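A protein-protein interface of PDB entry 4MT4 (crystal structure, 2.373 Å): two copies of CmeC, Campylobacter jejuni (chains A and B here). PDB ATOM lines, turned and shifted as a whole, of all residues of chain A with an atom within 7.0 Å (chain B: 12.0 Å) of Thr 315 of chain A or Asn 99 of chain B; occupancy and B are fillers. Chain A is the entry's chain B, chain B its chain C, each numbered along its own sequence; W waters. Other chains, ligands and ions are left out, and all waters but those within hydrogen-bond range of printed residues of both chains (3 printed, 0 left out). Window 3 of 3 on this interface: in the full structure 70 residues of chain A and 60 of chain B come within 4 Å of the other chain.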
ATOM      1  N   ASN A 112      -0.394  32.675   4.607  1.00  0.00           N
ATOM      2  CA  ASN A 112      -0.103  32.021   5.876  1.00  0.00           C
ATOM      3  C   ASN A 112       0.391  30.596   5.682  1.00  0.00           C
ATOM      4  O   ASN A 112       0.276  30.031   4.594  1.00  0.00           O
ATOM      5  CB  ASN A 112      -1.341  32.019   6.773  1.00  0.00           C
ATOM      6  CG  ASN A 112      -1.810  33.414   7.118  1.00  0.00           C
ATOM      7  OD1 ASN A 112      -1.011  34.343   7.209  1.00  0.00           O
ATOM      8  ND2 ASN A 112      -3.114  33.569   7.310  1.00  0.00           N
ATOM      9  N   ASP A 113       0.938  30.022   6.748  1.00  0.00           N
ATOM     10  CA  ASP A 113       1.407  28.642   6.731  1.00  0.00           C
ATOM     11  C   ASP A 113       1.373  28.047   8.134  1.00  0.00           C
ATOM     12  O   ASP A 113       2.092  28.493   9.028  1.00  0.00           O
ATOM     13  CB  ASP A 113       2.821  28.556   6.155  1.00  0.00           C
ATOM     14  CG  ASP A 113       3.253  27.129   5.878  1.00  0.00           C
ATOM     15  OD1 ASP A 113       2.384  26.294   5.545  1.00  0.00           O
ATOM     16  OD2 ASP A 113       4.463  26.841   5.991  1.00  0.00           O
ATOM     17  N   PHE A 308       0.359  17.687   9.653  1.00  0.00           N
ATOM     18  CA  PHE A 308      -0.557  18.531   8.896  1.00  0.00           C
ATOM     19  C   PHE A 308       0.089  19.819   8.387  1.00  0.00           C
ATOM     20  O   PHE A 308       1.032  20.338   8.987  1.00  0.00           O
ATOM     21  CB  PHE A 308      -1.776  18.881   9.755  1.00  0.00           C
ATOM     22  CG  PHE A 308      -2.518  17.683  10.283  1.00  0.00           C
ATOM     23  CD1 PHE A 308      -3.526  17.091   9.540  1.00  0.00           C
ATOM     24  CD2 PHE A 308      -2.213  17.155  11.529  1.00  0.00           C
ATOM     25  CE1 PHE A 308      -4.210  15.991  10.024  1.00  0.00           C
ATOM     26  CE2 PHE A 308      -2.894  16.054  12.018  1.00  0.00           C
ATOM     27  CZ  PHE A 308      -3.895  15.473  11.263  1.00  0.00           C
ATOM     28  N   GLU A 309      -0.429  20.327   7.272  1.00  0.00           N
ATOM     29  CA  GLU A 309      -0.044  21.640   6.764  1.00  0.00           C
ATOM     30  C   GLU A 309      -1.196  22.289   6.002  1.00  0.00           C
ATOM     31  O   GLU A 309      -1.842  21.655   5.172  1.00  0.00           O
ATOM     32  CB  GLU A 309       1.191  21.546   5.864  1.00  0.00           C
ATOM     33  CG  GLU A 309       1.661  22.898   5.345  1.00  0.00           C
ATOM     34  CD  GLU A 309       2.900  22.809   4.478  1.00  0.00           C
ATOM     35  OE1 GLU A 309       3.355  21.681   4.195  1.00  0.00           O
ATOM     36  OE2 GLU A 309       3.421  23.873   4.080  1.00  0.00           O
ATOM     37  N   SER A 310      -1.448  23.560   6.294  1.00  0.00           N
ATOM     38  CA  SER A 310      -2.502  24.306   5.620  1.00  0.00           C
ATOM     39  C   SER A 310      -2.202  25.801   5.615  1.00  0.00           C
ATOM     40  O   SER A 310      -1.466  26.301   6.464  1.00  0.00           O
ATOM     41  CB  SER A 310      -3.855  24.046   6.287  1.00  0.00           C
ATOM     42  OG  SER A 310      -4.888  24.793   5.662  1.00  0.00           O
ATOM     43  N   GLY A 311      -2.774  26.504   4.643  1.00  0.00           N
ATOM     44  CA  GLY A 311      -2.632  27.945   4.548  1.00  0.00           C
ATOM     45  C   GLY A 311      -3.634  28.651   5.439  1.00  0.00           C
ATOM     46  O   GLY A 311      -3.619  29.877   5.566  1.00  0.00           O
ATOM     47  N   ASP A 312      -4.511  27.863   6.052  1.00  0.00           N
ATOM     48  CA  ASP A 312      -5.512  28.385   6.970  1.00  0.00           C
ATOM     49  C   ASP A 312      -5.579  27.523   8.225  1.00  0.00           C
ATOM     50  O   ASP A 312      -5.480  26.296   8.156  1.00  0.00           O
ATOM     51  CB  ASP A 312      -6.884  28.448   6.297  1.00  0.00           C
ATOM     52  CG  ASP A 312      -6.836  29.121   4.938  1.00  0.00           C
ATOM     53  OD1 ASP A 312      -6.784  28.401   3.917  1.00  0.00           O
ATOM     54  OD2 ASP A 312      -6.849  30.369   4.886  1.00  0.00           O
ATOM     55  N   LEU A 313      -5.749  28.172   9.370  1.00  0.00           N
ATOM     56  CA  LEU A 313      -5.790  27.472  10.645  1.00  0.00           C
ATOM     57  C   LEU A 313      -7.059  26.633  10.789  1.00  0.00           C
ATOM     58  O   LEU A 313      -7.035  25.554  11.381  1.00  0.00           O
ATOM     59  CB  LEU A 313      -5.687  28.471  11.797  1.00  0.00           C
ATOM     60  CG  LEU A 313      -5.775  27.875  13.201  1.00  0.00           C
ATOM     61  CD1 LEU A 313      -4.655  26.872  13.423  1.00  0.00           C
ATOM     62  CD2 LEU A 313      -5.743  28.969  14.254  1.00  0.00           C
ATOM     63  N   ASP A 314      -8.161  27.126  10.236  1.00  0.00           N
ATOM     64  CA  ASP A 314      -9.454  26.465  10.393  1.00  0.00           C
ATOM     65  C   ASP A 314      -9.524  25.106   9.689  1.00  0.00           C
ATOM     66  O   ASP A 314     -10.372  24.280  10.021  1.00  0.00           O
ATOM     67  CB  ASP A 314     -10.578  27.375   9.888  1.00  0.00           C
ATOM     68  CG  ASP A 314     -10.393  27.785   8.443  1.00  0.00           C
ATOM     69  OD1 ASP A 314      -9.579  28.696   8.182  1.00  0.00           O
ATOM     70  OD2 ASP A 314     -11.072  27.203   7.571  1.00  0.00           O
ATOM     71  N   THR A 315      -8.634  24.876   8.728  1.00  0.00           N
ATOM     72  CA  THR A 315      -8.597  23.602   8.012  1.00  0.00           C
ATOM     73  C   THR A 315      -7.318  22.822   8.297  1.00  0.00           C
ATOM     74  O   THR A 315      -6.952  21.924   7.538  1.00  0.00           O
ATOM     75  CB  THR A 315      -8.709  23.799   6.488  1.00  0.00           C
ATOM     76  OG1 THR A 315      -7.615  24.603   6.025  1.00  0.00           O
ATOM     77  CG2 THR A 315     -10.023  24.473   6.126  1.00  0.00           C
ATOM     78  N   LEU A 316      -6.642  23.165   9.389  1.00  0.00           N
ATOM     79  CA  LEU A 316      -5.344  22.573   9.697  1.00  0.00           C
ATOM     80  C   LEU A 316      -5.418  21.065   9.938  1.00  0.00           C
ATOM     81  O   LEU A 316      -4.547  20.323   9.496  1.00  0.00           O
ATOM     82  CB  LEU A 316      -4.724  23.262  10.913  1.00  0.00           C
ATOM     83  CG  LEU A 316      -3.352  22.735  11.336  1.00  0.00           C
ATOM     84  CD1 LEU A 316      -2.364  22.840  10.186  1.00  0.00           C
ATOM     85  CD2 LEU A 316      -2.843  23.481  12.557  1.00  0.00           C
ATOM     86  N   VAL A 317      -6.453  20.610  10.635  1.00  0.00           N
ATOM     87  CA  VAL A 317      -6.570  19.189  10.953  1.00  0.00           C
ATOM     88  C   VAL A 317      -7.590  18.481  10.063  1.00  0.00           C
ATOM     89  O   VAL A 317      -8.067  17.395  10.392  1.00  0.00           O
ATOM     90  CB  VAL A 317      -6.949  18.968  12.431  1.00  0.00           C
ATOM     91  CG1 VAL A 317      -5.833  19.462  13.342  1.00  0.00           C
ATOM     92  CG2 VAL A 317      -8.260  19.660  12.757  1.00  0.00           C
ATOM     93  N   LYS A 318      -7.916  19.095   8.932  1.00  0.00           N
ATOM     94  CA  LYS A 318      -8.793  18.468   7.951  1.00  0.00           C
ATOM     95  C   LYS A 318      -8.052  17.370   7.195  1.00  0.00           C
ATOM     96  O   LYS A 318      -6.833  17.238   7.314  1.00  0.00           O
ATOM     97  CB  LYS A 318      -9.341  19.509   6.972  1.00  0.00           C
ATOM     98  CG  LYS A 318     -10.413  20.416   7.554  1.00  0.00           C
ATOM     99  CD  LYS A 318     -11.676  19.638   7.885  1.00  0.00           C
ATOM    100  CE  LYS A 318     -12.862  20.569   8.088  1.00  0.00           C
ATOM    101  NZ  LYS A 318     -12.621  21.556   9.177  1.00  0.00           N
ATOM    102  N   GLY A 319      -8.791  16.584   6.419  1.00  0.00           N
ATOM    103  CA  GLY A 319      -8.211  15.480   5.675  1.00  0.00           C
ATOM    104  C   GLY A 319      -7.257  15.935   4.588  1.00  0.00           C
ATOM    105  O   GLY A 319      -6.229  15.301   4.346  1.00  0.00           O
ATOM    106  N   GLY A 320      -7.597  17.041   3.934  1.00  0.00           N
ATOM    107  CA  GLY A 320      -6.780  17.584   2.864  1.00  0.00           C
ATOM    108  C   GLY A 320      -5.551  18.323   3.356  1.00  0.00           C
ATOM    109  O   GLY A 320      -4.845  18.961   2.574  1.00  0.00           O
ATOM    110  N   SER A 321      -5.295  18.244   4.656  1.00  0.00           N
ATOM    111  CA  SER A 321      -4.116  18.869   5.236  1.00  0.00           C
ATOM    112  C   SER A 321      -3.108  17.816   5.686  1.00  0.00           C
ATOM    113  O   SER A 321      -1.987  18.147   6.069  1.00  0.00           O
ATOM    114  CB  SER A 321      -4.503  19.770   6.410  1.00  0.00           C
ATOM    115  OG  SER A 321      -5.279  20.874   5.978  1.00  0.00           O
ATOM    116  N   LYS A 322      -3.509  16.548   5.631  1.00  0.00           N
ATOM    117  CA  LYS A 322      -2.618  15.451   6.000  1.00  0.00           C
ATOM    118  C   LYS A 322      -1.406  15.399   5.078  1.00  0.00           C
ATOM    119  O   LYS A 322      -1.536  15.499   3.858  1.00  0.00           O
ATOM    120  CB  LYS A 322      -3.355  14.111   5.969  1.00  0.00           C
ATOM    121  CG  LYS A 322      -4.342  13.923   7.107  1.00  0.00           C
ATOM    122  CD  LYS A 322      -4.758  12.467   7.248  1.00  0.00           C
ATOM    123  CE  LYS A 322      -5.537  11.987   6.035  1.00  0.00           C
ATOM    124  NZ  LYS A 322      -5.989  10.578   6.199  1.00  0.00           N
ATOM    125  N   LYS B  95       4.353  13.412   0.663  1.00  0.00           N
ATOM    126  CA  LYS B  95       2.953  13.584   0.313  1.00  0.00           C
ATOM    127  C   LYS B  95       2.530  14.995   0.686  1.00  0.00           C
ATOM    128  O   LYS B  95       2.197  15.267   1.839  1.00  0.00           O
ATOM    129  CB  LYS B  95       2.068  12.557   1.021  1.00  0.00           C
ATOM    130  CG  LYS B  95       0.592  12.694   0.677  1.00  0.00           C
ATOM    131  CD  LYS B  95      -0.277  11.717   1.453  1.00  0.00           C
ATOM    132  CE  LYS B  95      -0.587  12.227   2.850  1.00  0.00           C
ATOM    133  NZ  LYS B  95      -1.478  11.285   3.584  1.00  0.00           N
ATOM    134  N   THR B  96       2.558  15.895  -0.287  1.00  0.00           N
ATOM    135  CA  THR B  96       2.193  17.283  -0.039  1.00  0.00           C
ATOM    136  C   THR B  96       0.680  17.429   0.046  1.00  0.00           C
ATOM    137  O   THR B  96      -0.047  17.010  -0.854  1.00  0.00           O
ATOM    138  CB  THR B  96       2.747  18.216  -1.128  1.00  0.00           C
ATOM    139  OG1 THR B  96       4.173  18.088  -1.182  1.00  0.00           O
ATOM    140  CG2 THR B  96       2.388  19.660  -0.821  1.00  0.00           C
ATOM    141  N   ALA B  97       0.217  18.019   1.141  1.00  0.00           N
ATOM    142  CA  ALA B  97      -1.210  18.155   1.402  1.00  0.00           C
ATOM    143  C   ALA B  97      -1.903  19.033   0.366  1.00  0.00           C
ATOM    144  O   ALA B  97      -1.267  19.865  -0.284  1.00  0.00           O
ATOM    145  CB  ALA B  97      -1.433  18.716   2.796  1.00  0.00           C
ATOM    146  N   ILE B  98      -3.209  18.831   0.214  1.00  0.00           N
ATOM    147  CA  ILE B  98      -4.021  19.652  -0.677  1.00  0.00           C
ATOM    148  C   ILE B  98      -4.032  21.103  -0.207  1.00  0.00           C
ATOM    149  O   ILE B  98      -3.958  22.033  -1.011  1.00  0.00           O
ATOM    150  CB  ILE B  98      -5.476  19.133  -0.755  1.00  0.00           C
ATOM    151  CG1 ILE B  98      -5.501  17.687  -1.253  1.00  0.00           C
ATOM    152  CG2 ILE B  98      -6.325  20.023  -1.651  1.00  0.00           C
ATOM    153  CD1 ILE B  98      -6.896  17.115  -1.378  1.00  0.00           C
ATOM    154  N   ASN B  99      -4.110  21.284   1.108  1.00  0.00           N
ATOM    155  CA  ASN B  99      -4.208  22.609   1.704  1.00  0.00           C
ATOM    156  C   ASN B  99      -2.861  23.303   1.863  1.00  0.00           C
ATOM    157  O   ASN B  99      -2.799  24.452   2.297  1.00  0.00           O
ATOM    158  CB  ASN B  99      -4.901  22.521   3.065  1.00  0.00           C
ATOM    159  CG  ASN B  99      -6.338  22.055   2.958  1.00  0.00           C
ATOM    160  OD1 ASN B  99      -6.996  22.265   1.939  1.00  0.00           O
ATOM    161  ND2 ASN B  99      -6.835  21.417   4.012  1.00  0.00           N
ATOM    162  N   ALA B 100      -1.786  22.606   1.514  1.00  0.00           N
ATOM    163  CA  ALA B 100      -0.454  23.193   1.578  1.00  0.00           C
ATOM    164  C   ALA B 100      -0.336  24.339   0.577  1.00  0.00           C
ATOM    165  O   ALA B 100      -0.708  24.188  -0.587  1.00  0.00           O
ATOM    166  CB  ALA B 100       0.609  22.139   1.316  1.00  0.00           C
ATOM    167  N   PRO B 101       0.179  25.493   1.032  1.00  0.00           N
ATOM    168  CA  PRO B 101       0.311  26.713   0.223  1.00  0.00           C
ATOM    169  C   PRO B 101       1.045  26.487  -1.099  1.00  0.00           C
ATOM    170  O   PRO B 101       0.700  27.103  -2.108  1.00  0.00           O
ATOM    171  CB  PRO B 101       1.117  27.647   1.130  1.00  0.00           C
ATOM    172  CG  PRO B 101       0.820  27.179   2.503  1.00  0.00           C
ATOM    173  CD  PRO B 101       0.669  25.691   2.408  1.00  0.00           C
ATOM    174  N   SER B 102       2.043  25.611  -1.091  1.00  0.00           N
ATOM    175  CA  SER B 102       2.832  25.350  -2.289  1.00  0.00           C
ATOM    176  C   SER B 102       2.049  24.516  -3.298  1.00  0.00           C
ATOM    177  O   SER B 102       2.358  24.518  -4.492  1.00  0.00           O
ATOM    178  CB  SER B 102       4.141  24.646  -1.927  1.00  0.00           C
ATOM    179  OG  SER B 102       3.899  23.377  -1.344  1.00  0.00           O
ATOM    180  N   ASN B 103       1.031  23.810  -2.816  1.00  0.00           N
ATOM    181  CA  ASN B 103       0.220  22.956  -3.675  1.00  0.00           C
ATOM    182  C   ASN B 103      -0.995  23.688  -4.239  1.00  0.00           C
ATOM    183  O   ASN B 103      -1.928  24.021  -3.507  1.00  0.00           O
ATOM    184  CB  ASN B 103      -0.228  21.709  -2.908  1.00  0.00           C
ATOM    185  CG  ASN B 103      -0.870  20.669  -3.806  1.00  0.00           C
ATOM    186  OD1 ASN B 103      -0.821  20.772  -5.031  1.00  0.00           O
ATOM    187  ND2 ASN B 103      -1.469  19.652  -3.196  1.00  0.00           N
ATOM    188  N   ARG B 104      -0.975  23.928  -5.546  1.00  0.00           N
ATOM    189  CA  ARG B 104      -2.049  24.644  -6.224  1.00  0.00           C
ATOM    190  C   ARG B 104      -2.736  23.762  -7.259  1.00  0.00           C
ATOM    191  O   ARG B 104      -3.334  24.258  -8.216  1.00  0.00           O
ATOM    192  CB  ARG B 104      -1.503  25.915  -6.880  1.00  0.00           C
ATOM    193  CG  ARG B 104      -0.080  25.773  -7.401  1.00  0.00           C
ATOM    194  CD  ARG B 104       0.542  27.132  -7.687  1.00  0.00           C
ATOM    195  NE  ARG B 104       1.996  27.055  -7.821  1.00  0.00           N
ATOM    196  CZ  ARG B 104       2.846  27.163  -6.805  1.00  0.00           C
ATOM    197  NH1 ARG B 104       2.391  27.348  -5.573  1.00  0.00           N
ATOM    198  NH2 ARG B 104       4.153  27.086  -7.019  1.00  0.00           N
ATOM    199  N   THR B 105      -2.648  22.452  -7.059  1.00  0.00           N
ATOM    200  CA  THR B 105      -3.247  21.492  -7.979  1.00  0.00           C
ATOM    201  C   THR B 105      -4.650  21.098  -7.524  1.00  0.00           C
ATOM    202  O   THR B 105      -5.452  20.601  -8.313  1.00  0.00           O
ATOM    203  CB  THR B 105      -2.381  20.225  -8.112  1.00  0.00           C
ATOM    204  OG1 THR B 105      -2.323  19.547  -6.850  1.00  0.00           O
ATOM    205  CG2 THR B 105      -0.970  20.587  -8.553  1.00  0.00           C
ATOM    206  N   GLY B 106      -4.937  21.321  -6.246  1.00  0.00           N
ATOM    207  CA  GLY B 106      -6.244  21.019  -5.694  1.00  0.00           C
ATOM    208  C   GLY B 106      -6.385  19.569  -5.280  1.00  0.00           C
ATOM    209  O   GLY B 106      -7.455  19.138  -4.846  1.00  0.00           O
ATOM    210  N   GLU B 107      -5.298  18.814  -5.408  1.00  0.00           N
ATOM    211  CA  GLU B 107      -5.309  17.397  -5.065  1.00  0.00           C
ATOM    212  C   GLU B 107      -4.005  16.977  -4.393  1.00  0.00           C
ATOM    213  O   GLU B 107      -2.999  17.685  -4.473  1.00  0.00           O
ATOM    214  CB  GLU B 107      -5.566  16.554  -6.317  1.00  0.00           C
ATOM    215  CG  GLU B 107      -4.806  17.020  -7.553  1.00  0.00           C
ATOM    216  CD  GLU B 107      -5.394  16.468  -8.838  1.00  0.00           C
ATOM    217  OE1 GLU B 107      -6.335  15.649  -8.757  1.00  0.00           O
ATOM    218  OE2 GLU B 107      -4.923  16.855  -9.928  1.00  0.00           O
ATOM    219  N   VAL B 108      -4.038  15.830  -3.718  1.00  0.00           N
ATOM    220  CA  VAL B 108      -2.864  15.294  -3.034  1.00  0.00           C
ATOM    221  C   VAL B 108      -1.703  15.062  -4.001  1.00  0.00           C
ATOM    222  O   VAL B 108      -1.867  14.422  -5.039  1.00  0.00           O
ATOM    223  CB  VAL B 108      -3.199  13.972  -2.311  1.00  0.00           C
ATOM    224  CG1 VAL B 108      -1.947  13.338  -1.737  1.00  0.00           C
ATOM    225  CG2 VAL B 108      -4.228  14.213  -1.218  1.00  0.00           C
ATOM    226  N   SER B 109      -0.531  15.589  -3.654  1.00  0.00           N
ATOM    227  CA  SER B 109       0.628  15.515  -4.537  1.00  0.00           C
ATOM    228  C   SER B 109       1.772  14.689  -3.950  1.00  0.00           C
ATOM    229  O   SER B 109       2.327  15.031  -2.908  1.00  0.00           O
ATOM    230  CB  SER B 109       1.125  16.926  -4.863  1.00  0.00           C
ATOM    231  OG  SER B 109       2.238  16.891  -5.740  1.00  0.00           O
ATOM    232  N   TYR B 110       2.119  13.601  -4.630  1.00  0.00           N
ATOM    233  CA  TYR B 110       3.281  12.800  -4.263  1.00  0.00           C
ATOM    234  C   TYR B 110       4.458  13.172  -5.157  1.00  0.00           C
ATOM    235  O   TYR B 110       4.314  13.238  -6.377  1.00  0.00           O
ATOM    236  CB  TYR B 110       2.979  11.304  -4.382  1.00  0.00           C
ATOM    237  CG  TYR B 110       1.835  10.829  -3.517  1.00  0.00           C
ATOM    238  CD1 TYR B 110       0.530  10.834  -3.992  1.00  0.00           C
ATOM    239  CD2 TYR B 110       2.059  10.368  -2.225  1.00  0.00           C
ATOM    240  CE1 TYR B 110      -0.520  10.398  -3.207  1.00  0.00           C
ATOM    241  CE2 TYR B 110       1.015   9.930  -1.432  1.00  0.00           C
ATOM    242  CZ  TYR B 110      -0.272   9.948  -1.928  1.00  0.00           C
ATOM    243  OH  TYR B 110      -1.315   9.514  -1.145  1.00  0.00           O
HETATM  244  O   HOH W   1       3.675  24.847   1.338  1.00  0.00           O
HETATM  245  O   HOH W   2       2.247  19.350   2.830  1.00  0.00           O
HETATM  246  O   HOH W   3      -4.958  26.255   2.484  1.00  0.00           O
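The backbone carbonyl oxygen (O) of Asn 99 of chain B sits at hydrogen-bond distance from the backbone NH (N) of Gly 311 of chain A (3.1 Å). The backbone carbonyl oxygen (O) of Gly 320 of chain A lies within hydrogen-bond range of the backbone NH (N) of Ile 98 of chain B. The backbone NH (N) of Asn 99 of chain B is in hydrogen-bond range of the backbone carbonyl oxygen (O) of Gly 320 of chain A. OG of Ser 321 of chain A is in hydrogen-bond range of ND2 of Asn 99 of chain B.
The backbone NH (N) of Glu 309 of chain A sits at hydrogen-bond distance from the backbone carbonyl oxygen (O) of Ser 321 of chain A, at 2.9 Å. The side-chain hydroxyl of Ser 310 of chain A is in hydrogen-bond range of the backbone carbonyl oxygen of Asp 312 of chain A (3.0 Å). OG of Ser 310 of chain A lies within hydrogen-bond range of OG1 of Thr 315 of chain A (2.8 Å). The backbone carbonyl oxygen (O) of Asp 312 of chain A lies within hydrogen-bond range of the side-chain hydroxyl (OG1) of Thr 315 of chain A (3.5 Å). OG of Ser 321 of chain A sits at hydrogen-bond distance from O of Thr 315 of chain A, at 2.5 Å. The side-chain amide nitrogen (ND2) of Asn 103 of chain B is in hydrogen-bond range of the backbone carbonyl oxygen (O) of Ala 97 of chain B (2.9 Å).
Among the printed residues, merely in contact across the chains: Ser 310 of chain A with Asn 99 of chain B (3.3 Å), Ser 321 of chain A with Ala 97 of chain B (3.4 Å), Lys 322 of chain A with Ala 97 of chain B (3.4 Å), Gly 320 of chain A with Ala 97 of chain B (3.4 Å), Asp 113 of chain A with Pro 101 of chain B (3.5 Å), Lys 322 of chain A with Lys 95 of chain B (3.6 Å), Thr 315 of chain A with Asn 99 of chain B (3.6 Å), Asn 112 of chain A with Pro 101 of chain B (3.6 Å), Glu 309 of chain A with Pro 101 of chain B (3.7 Å), Glu 309 of chain A with Ala 100 of chain B (3.8 Å), Glu 309 of chain A with Ala 97 of chain B (3.8 Å) and Glu 309 of chain A with Asn 99 of chain B (3.8 Å).
Of the printed residues of chain B, Asn 112 of chain A touches Pro 101 (3.6 Å). Of the printed residues of chain B, Asp 113 of chain A touches Pro 101 (3.5 Å). Glu 309 of chain A touches four residues of chain B. Of chain B, only Asn 99 (3.3 Å) comes within 4 Å of Ser 310 of chain A. No residue of chain B comes within 4 Å of Leu 313 of chain A. Of chain B, only Asn 99 (3.6 Å) comes within 4 Å of Thr 315 of chain A. Val 317 of chain A touches none of the printed residues of chain B. No residue of chain B comes within 4 Å of Lys 318 of chain A. Gly 320 of chain A touches just these residues of chain B: Ala 97, Ile 98 and Asn 99. Ser 321 of chain A touches just these residues of chain B: Ala 97 (3.4 Å) and Asn 99 (2.6 Å). Printed residues of chain A within 4 Å of Lys 95 of chain B: Lys 322. Of the printed residues of chain A, Ile 98 of chain B touches Gly 320. Asn 99 of chain B touches just these residues of chain A: Glu 309, Ser 310, Gly 311, Thr 315, Gly 320 and Ser 321. Ser 102 of chain B touches none of the printed residues of chain A. The nearest residue of chain A that does not touch Asn 99 of chain B is Lys 318 of chain A (4.3 Å). The nearest printed residue of chain B that does not touch Asn 112 of chain A is Asn 99 of chain B (6.8 Å).
Of the 16 printed residues of chain B, 6 touch a printed residue of chain A. Hydrophobic or aromatic side chains of chain B within 4 Å of the printed part of chain A: Ala 97, Ile 98, Ala 100 and Pro 101. Along chain B the printed residues that touch a printed residue of chain A span positions 95 to 101. Printed residues of chain A that touch a printed residue of chain B: Asn 112, Asp 113, Glu 309, Ser 310, Gly 311, Thr 315, Gly 320, Ser 321 and Lys 322.
No position is printed for both chains. Of the 16 pairs that touch across the chains among the printed residues, none has its exchanged pair printed and touching as well.
Water W3 lies within hydrogen-bond range of O of Asn 99 of chain B, N of Gly 311 of chain A, OD1 of Asp 312 of chain A and OG of Ser 310 of chain A. Water W2 bridges OE1 of Glu 309 of chain A (2.9 Å) and N of Ala 97 of chain B (3.0 Å). Water W1 lies within hydrogen-bond range of the side-chain carboxylate of Glu 309 of chain A (2.9 Å) and the backbone NH of Ser 102 of chain B (3.0 Å).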
